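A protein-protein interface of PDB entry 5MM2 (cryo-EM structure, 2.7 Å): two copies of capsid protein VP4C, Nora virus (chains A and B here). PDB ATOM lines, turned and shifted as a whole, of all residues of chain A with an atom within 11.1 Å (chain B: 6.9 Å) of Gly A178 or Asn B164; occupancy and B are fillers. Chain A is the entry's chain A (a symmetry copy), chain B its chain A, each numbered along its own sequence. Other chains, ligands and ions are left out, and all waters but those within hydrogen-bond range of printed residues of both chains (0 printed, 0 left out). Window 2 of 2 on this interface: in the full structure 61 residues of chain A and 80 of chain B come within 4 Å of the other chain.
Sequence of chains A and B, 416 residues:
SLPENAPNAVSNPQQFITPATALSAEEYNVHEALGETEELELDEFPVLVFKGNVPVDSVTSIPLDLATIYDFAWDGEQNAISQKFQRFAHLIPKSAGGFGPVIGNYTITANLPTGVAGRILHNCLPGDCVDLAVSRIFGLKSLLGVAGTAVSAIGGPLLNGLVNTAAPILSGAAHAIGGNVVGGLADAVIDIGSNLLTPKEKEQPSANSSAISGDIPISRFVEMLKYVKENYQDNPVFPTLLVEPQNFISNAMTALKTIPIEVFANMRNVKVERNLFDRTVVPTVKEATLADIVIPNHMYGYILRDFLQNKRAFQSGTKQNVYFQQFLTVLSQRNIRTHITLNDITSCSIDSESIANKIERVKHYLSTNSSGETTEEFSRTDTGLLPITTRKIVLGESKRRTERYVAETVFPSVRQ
The side-chain hydroxyl (OG1) of Thr B107 is in hydrogen-bond range of the backbone NH (N) of Ile A177, 3.1 Å away. N of Ala B211 sits at hydrogen-bond distance from O of Asn A180 (3.0 Å).
The backbone carbonyl oxygen (O) of Leu B162 lies within hydrogen-bond range of the side-chain hydroxyl (OG) of Ser B209 (2.5 Å). O of Ser B206 sits at hydrogen-bond distance from ND2 of Asn B164 (3.3 Å).
Among the printed residues, merely in contact across the chains: Gln A204 with Asn B208, Gln A204 with Ser B209, Gly A179 with Ala B211, Gly A178 with Asn B164, Gly A178 with Leu B162 and Ala A176 with Thr B107.
Of chain B, only Leu B162 and Asn B164 come within 4 Å of Gly A178. Of the printed residues of chain A, Asn B164 touches Gly A178. Leu B162 touches just one residue of chain A: Gly A178 (3.9 Å). No residue of chain A comes within 4 Å of Thr B165. No residue of chain A comes within 4 Å of Ala B166. No residue of chain A comes within 4 Å of Ala B207. Ser B209 touches just one residue of chain A: Gln A204 (3.7 Å). Of the printed residues of chain B, Gly A179 touches Ala B211. Of the printed residues of chain A, Ala B211 touches Gly A179 and Asn A180. Val A182 touches none of the printed residues of chain B. Val B182 touches none of the printed residues of chain A. The nearest residue of chain A that does not touch Asn B164 is Gly A179 (5.7 Å). The nearest printed residue of chain B that does not touch Gly A179 is Ser B209 (4.1 Å).
Hydrophobic or aromatic side chains of chain B that line the printed part of chain A: Ala B211. Printed residues of chain A that touch a printed residue of chain B: Ala A176, Ile A177, Gly A178, Gly A179, Asn A180 and Gln A204. Among the printed residues, 8 pairs touch across the chains. Among the printed residues, no Asp or Glu carboxylate lies within 4 Å of a Lys or Arg side-chain nitrogen of the other chain.
Positions printed for both chains: 182 and 206. Of the 8 pairs that touch across the chains among the printed residues, none has its exchanged pair printed and touching as well.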
ATOM      1  N   ALA A 173      -4.853  17.924  17.224  1.00  0.00           N
ATOM      2  CA  ALA A 173      -4.503  16.944  16.194  1.00  0.00           C
ATOM      3  C   ALA A 173      -4.072  15.617  16.816  1.00  0.00           C
ATOM      4  O   ALA A 173      -2.969  15.123  16.604  1.00  0.00           O
ATOM      5  CB  ALA A 173      -3.438  17.493  15.246  1.00  0.00           C
ATOM      6  N   ALA A 174      -4.985  15.040  17.593  1.00  0.00           N
ATOM      7  CA  ALA A 174      -4.701  13.797  18.292  1.00  0.00           C
ATOM      8  C   ALA A 174      -4.730  12.579  17.384  1.00  0.00           C
ATOM      9  O   ALA A 174      -4.266  11.515  17.797  1.00  0.00           O
ATOM     10  CB  ALA A 174      -5.694  13.603  19.431  1.00  0.00           C
ATOM     11  N   HIS A 175      -5.260  12.698  16.174  1.00  0.00           N
ATOM     12  CA  HIS A 175      -5.235  11.617  15.198  1.00  0.00           C
ATOM     13  C   HIS A 175      -4.345  12.084  14.057  1.00  0.00           C
ATOM     14  O   HIS A 175      -4.819  12.510  13.008  1.00  0.00           O
ATOM     15  CB  HIS A 175      -6.615  11.304  14.712  1.00  0.00           C
ATOM     16  CG  HIS A 175      -7.539  10.811  15.775  1.00  0.00           C
ATOM     17  ND1 HIS A 175      -8.889  10.662  15.572  1.00  0.00           N
ATOM     18  CD2 HIS A 175      -7.306  10.434  17.052  1.00  0.00           C
ATOM     19  CE1 HIS A 175      -9.452  10.216  16.678  1.00  0.00           C
ATOM     20  NE2 HIS A 175      -8.511  10.064  17.591  1.00  0.00           N
ATOM     21  N   ALA A 176      -3.042  11.972  14.251  1.00  0.00           N
ATOM     22  CA  ALA A 176      -2.079  12.375  13.246  1.00  0.00           C
ATOM     23  C   ALA A 176      -1.297  11.148  12.825  1.00  0.00           C
ATOM     24  O   ALA A 176      -0.945  10.316  13.662  1.00  0.00           O
ATOM     25  CB  ALA A 176      -1.143  13.455  13.770  1.00  0.00           C
ATOM     26  N   ILE A 177      -1.031  11.026  11.532  1.00  0.00           N
ATOM     27  CA  ILE A 177      -0.504   9.787  10.982  1.00  0.00           C
ATOM     28  C   ILE A 177       1.015   9.839  11.021  1.00  0.00           C
ATOM     29  O   ILE A 177       1.638  10.659  10.347  1.00  0.00           O
ATOM     30  CB  ILE A 177      -1.015   9.518   9.563  1.00  0.00           C
ATOM     31  CG1 ILE A 177      -2.530   9.311   9.542  1.00  0.00           C
ATOM     32  CG2 ILE A 177      -0.340   8.300   8.997  1.00  0.00           C
ATOM     33  CD1 ILE A 177      -3.339  10.533   9.183  1.00  0.00           C
ATOM     34  N   GLY A 178       1.609   8.960  11.817  1.00  0.00           N
ATOM     35  CA  GLY A 178       3.031   8.710  11.745  1.00  0.00           C
ATOM     36  C   GLY A 178       3.901   9.657  12.524  1.00  0.00           C
ATOM     37  O   GLY A 178       5.116   9.665  12.323  1.00  0.00           O
ATOM     38  N   GLY A 179       3.328  10.457  13.408  1.00  0.00           N
ATOM     39  CA  GLY A 179       4.138  11.372  14.174  1.00  0.00           C
ATOM     40  C   GLY A 179       3.326  12.247  15.092  1.00  0.00           C
ATOM     41  O   GLY A 179       2.109  12.353  14.947  1.00  0.00           O
ATOM     42  N   ASN A 180       3.990  12.886  16.040  1.00  0.00           N
ATOM     43  CA  ASN A 180       3.328  13.690  17.049  1.00  0.00           C
ATOM     44  C   ASN A 180       3.449  15.164  16.714  1.00  0.00           C
ATOM     45  O   ASN A 180       4.509  15.630  16.298  1.00  0.00           O
ATOM     46  CB  ASN A 180       3.935  13.418  18.420  1.00  0.00           C
ATOM     47  CG  ASN A 180       3.521  12.091  18.976  1.00  0.00           C
ATOM     48  OD1 ASN A 180       2.340  11.759  18.996  1.00  0.00           O
ATOM     49  ND2 ASN A 180       4.494  11.294  19.388  1.00  0.00           N
ATOM     50  N   VAL A 181       2.354  15.887  16.885  1.00  0.00           N
ATOM     51  CA  VAL A 181       2.390  17.340  16.806  1.00  0.00           C
ATOM     52  C   VAL A 181       3.070  17.853  18.063  1.00  0.00           C
ATOM     53  O   VAL A 181       2.616  17.594  19.180  1.00  0.00           O
ATOM     54  CB  VAL A 181       0.983  17.922  16.656  1.00  0.00           C
ATOM     55  CG1 VAL A 181       1.049  19.424  16.683  1.00  0.00           C
ATOM     56  CG2 VAL A 181       0.375  17.449  15.368  1.00  0.00           C
ATOM     57  N   VAL A 182       4.156  18.584  17.883  1.00  0.00           N
ATOM     58  CA  VAL A 182       5.059  18.921  18.967  1.00  0.00           C
ATOM     59  C   VAL A 182       4.713  20.301  19.485  1.00  0.00           C
ATOM     60  O   VAL A 182       4.822  21.293  18.757  1.00  0.00           O
ATOM     61  CB  VAL A 182       6.518  18.852  18.510  1.00  0.00           C
ATOM     62  CG1 VAL A 182       7.424  19.316  19.606  1.00  0.00           C
ATOM     63  CG2 VAL A 182       6.847  17.444  18.101  1.00  0.00           C
ATOM     64  N   LYS A 200       6.951  17.490  25.005  1.00  0.00           N
ATOM     65  CA  LYS A 200       7.293  16.827  23.759  1.00  0.00           C
ATOM     66  C   LYS A 200       8.353  17.553  22.961  1.00  0.00           C
ATOM     67  O   LYS A 200       8.938  16.952  22.059  1.00  0.00           O
ATOM     68  CB  LYS A 200       6.064  16.665  22.862  1.00  0.00           C
ATOM     69  CG  LYS A 200       5.060  15.655  23.338  1.00  0.00           C
ATOM     70  CD  LYS A 200       3.956  15.500  22.323  1.00  0.00           C
ATOM     71  CE  LYS A 200       2.883  14.569  22.815  1.00  0.00           C
ATOM     72  NZ  LYS A 200       3.361  13.184  22.942  1.00  0.00           N
ATOM     73  N   GLN A 204      12.386  16.125  20.823  1.00  0.00           N
ATOM     74  CA  GLN A 204      12.152  16.307  19.398  1.00  0.00           C
ATOM     75  C   GLN A 204      13.305  16.899  18.578  1.00  0.00           C
ATOM     76  O   GLN A 204      13.484  16.511  17.413  1.00  0.00           O
ATOM     77  CB  GLN A 204      10.879  17.135  19.220  1.00  0.00           C
ATOM     78  CG  GLN A 204      10.507  17.323  17.780  1.00  0.00           C
ATOM     79  CD  GLN A 204      10.462  15.999  17.047  1.00  0.00           C
ATOM     80  OE1 GLN A 204       9.814  15.051  17.482  1.00  0.00           O
ATOM     81  NE2 GLN A 204      11.241  15.902  15.977  1.00  0.00           N
ATOM     82  N   SER A 206      14.129  19.042  16.530  1.00  0.00           N
ATOM     83  CA  SER A 206      13.805  19.674  15.254  1.00  0.00           C
ATOM     84  C   SER A 206      12.685  20.698  15.366  1.00  0.00           C
ATOM     85  O   SER A 206      12.700  21.706  14.659  1.00  0.00           O
ATOM     86  CB  SER A 206      13.417  18.615  14.230  1.00  0.00           C
ATOM     87  OG  SER A 206      14.515  17.776  13.950  1.00  0.00           O
ATOM     88  N   THR B 107      -1.768  15.071   7.683  1.00  0.00           N
ATOM     89  CA  THR B 107      -0.334  15.046   7.933  1.00  0.00           C
ATOM     90  C   THR B 107       0.381  15.314   6.624  1.00  0.00           C
ATOM     91  O   THR B 107       0.175  14.595   5.647  1.00  0.00           O
ATOM     92  CB  THR B 107       0.112  13.708   8.513  1.00  0.00           C
ATOM     93  OG1 THR B 107      -0.563  13.481   9.751  1.00  0.00           O
ATOM     94  CG2 THR B 107       1.591  13.712   8.776  1.00  0.00           C
ATOM     95  N   LEU B 162       8.394  13.755   8.400  1.00  0.00           N
ATOM     96  CA  LEU B 162       8.903  12.411   8.168  1.00  0.00           C
ATOM     97  C   LEU B 162       7.960  11.423   8.827  1.00  0.00           C
ATOM     98  O   LEU B 162       7.327  11.733   9.838  1.00  0.00           O
ATOM     99  CB  LEU B 162      10.320  12.217   8.728  1.00  0.00           C
ATOM    100  CG  LEU B 162      11.534  13.010   8.238  1.00  0.00           C
ATOM    101  CD1 LEU B 162      12.738  12.717   9.085  1.00  0.00           C
ATOM    102  CD2 LEU B 162      11.841  12.724   6.800  1.00  0.00           C
ATOM    103  N   VAL B 163       7.875  10.228   8.254  1.00  0.00           N
ATOM    104  CA  VAL B 163       6.963   9.188   8.712  1.00  0.00           C
ATOM    105  C   VAL B 163       7.784   7.964   9.087  1.00  0.00           C
ATOM    106  O   VAL B 163       8.600   7.494   8.289  1.00  0.00           O
ATOM    107  CB  VAL B 163       5.921   8.841   7.637  1.00  0.00           C
ATOM    108  CG1 VAL B 163       5.041   7.713   8.100  1.00  0.00           C
ATOM    109  CG2 VAL B 163       5.076  10.042   7.316  1.00  0.00           C
ATOM    110  N   ASN B 164       7.585   7.464  10.301  1.00  0.00           N
ATOM    111  CA  ASN B 164       8.238   6.256  10.785  1.00  0.00           C
ATOM    112  C   ASN B 164       7.203   5.406  11.493  1.00  0.00           C
ATOM    113  O   ASN B 164       6.611   5.848  12.481  1.00  0.00           O
ATOM    114  CB  ASN B 164       9.384   6.597  11.729  1.00  0.00           C
ATOM    115  CG  ASN B 164      10.529   7.243  11.021  1.00  0.00           C
ATOM    116  OD1 ASN B 164      10.936   6.803   9.954  1.00  0.00           O
ATOM    117  ND2 ASN B 164      11.045   8.313  11.593  1.00  0.00           N
ATOM    118  N   THR B 165       6.995   4.190  11.001  1.00  0.00           N
ATOM    119  CA  THR B 165       5.857   3.377  11.401  1.00  0.00           C
ATOM    120  C   THR B 165       6.213   2.294  12.407  1.00  0.00           C
ATOM    121  O   THR B 165       5.534   2.187  13.433  1.00  0.00           O
ATOM    122  CB  THR B 165       5.210   2.754  10.165  1.00  0.00           C
ATOM    123  OG1 THR B 165       4.779   3.799   9.291  1.00  0.00           O
ATOM    124  CG2 THR B 165       4.009   1.906  10.547  1.00  0.00           C
ATOM    125  N   ALA B 166       7.250   1.492  12.124  1.00  0.00           N
ATOM    126  CA  ALA B 166       7.711   0.397  12.980  1.00  0.00           C
ATOM    127  C   ALA B 166       6.630  -0.652  13.216  1.00  0.00           C
ATOM    128  O   ALA B 166       5.975  -0.638  14.259  1.00  0.00           O
ATOM    129  CB  ALA B 166       8.272   0.910  14.310  1.00  0.00           C
ATOM    130  N   VAL B 182      12.255   1.326  17.165  1.00  0.00           N
ATOM    131  CA  VAL B 182      11.924   2.439  18.034  1.00  0.00           C
ATOM    132  C   VAL B 182      10.424   2.645  18.019  1.00  0.00           C
ATOM    133  O   VAL B 182       9.842   2.964  16.978  1.00  0.00           O
ATOM    134  CB  VAL B 182      12.660   3.710  17.606  1.00  0.00           C
ATOM    135  CG1 VAL B 182      12.216   4.870  18.440  1.00  0.00           C
ATOM    136  CG2 VAL B 182      14.143   3.495  17.734  1.00  0.00           C
ATOM    137  N   PRO B 205      16.236  10.609  18.489  1.00  0.00           N
ATOM    138  CA  PRO B 205      15.154  11.327  17.803  1.00  0.00           C
ATOM    139  C   PRO B 205      15.004  11.263  16.283  1.00  0.00           C
ATOM    140  O   PRO B 205      14.086  11.916  15.803  1.00  0.00           O
ATOM    141  CB  PRO B 205      15.450  12.784  18.155  1.00  0.00           C
ATOM    142  CG  PRO B 205      16.296  12.742  19.321  1.00  0.00           C
ATOM    143  CD  PRO B 205      17.144  11.562  19.135  1.00  0.00           C
ATOM    144  N   SER B 206      15.890  10.583  15.551  1.00  0.00           N
ATOM    145  CA  SER B 206      15.649  10.300  14.139  1.00  0.00           C
ATOM    146  C   SER B 206      14.318   9.607  13.890  1.00  0.00           C
ATOM    147  O   SER B 206      13.680   9.847  12.864  1.00  0.00           O
ATOM    148  CB  SER B 206      16.775   9.439  13.580  1.00  0.00           C
ATOM    149  OG  SER B 206      17.994  10.147  13.604  1.00  0.00           O
ATOM    150  N   ALA B 207      13.875   8.756  14.807  1.00  0.00           N
ATOM    151  CA  ALA B 207      12.596   8.082  14.667  1.00  0.00           C
ATOM    152  C   ALA B 207      11.471   8.776  15.419  1.00  0.00           C
ATOM    153  O   ALA B 207      10.388   8.202  15.549  1.00  0.00           O
ATOM    154  CB  ALA B 207      12.712   6.637  15.138  1.00  0.00           C
ATOM    155  N   ASN B 208      11.689   9.991  15.917  1.00  0.00           N
ATOM    156  CA  ASN B 208      10.639  10.674  16.660  1.00  0.00           C
ATOM    157  C   ASN B 208       9.823  11.590  15.754  1.00  0.00           C
ATOM    158  O   ASN B 208       8.593  11.551  15.807  1.00  0.00           O
ATOM    159  CB  ASN B 208      11.236  11.455  17.826  1.00  0.00           C
ATOM    160  CG  ASN B 208      10.206  11.840  18.852  1.00  0.00           C
ATOM    161  OD1 ASN B 208       9.032  11.504  18.732  1.00  0.00           O
ATOM    162  ND2 ASN B 208      10.643  12.542  19.882  1.00  0.00           N
ATOM    163  N   SER B 209      10.495  12.415  14.942  1.00  0.00           N
ATOM    164  CA  SER B 209       9.929  13.037  13.738  1.00  0.00           C
ATOM    165  C   SER B 209       8.751  13.968  14.043  1.00  0.00           C
ATOM    166  O   SER B 209       7.589  13.593  13.906  1.00  0.00           O
ATOM    167  CB  SER B 209       9.511  11.977  12.724  1.00  0.00           C
ATOM    168  OG  SER B 209       8.888  12.613  11.630  1.00  0.00           O
ATOM    169  N   ALA B 211       5.928  16.178  13.746  1.00  0.00           N
ATOM    170  CA  ALA B 211       5.058  16.107  12.585  1.00  0.00           C
ATOM    171  C   ALA B 211       4.494  17.471  12.196  1.00  0.00           C
ATOM    172  O   ALA B 211       4.493  18.426  12.973  1.00  0.00           O
ATOM    173  CB  ALA B 211       3.913  15.139  12.848  1.00  0.00           C
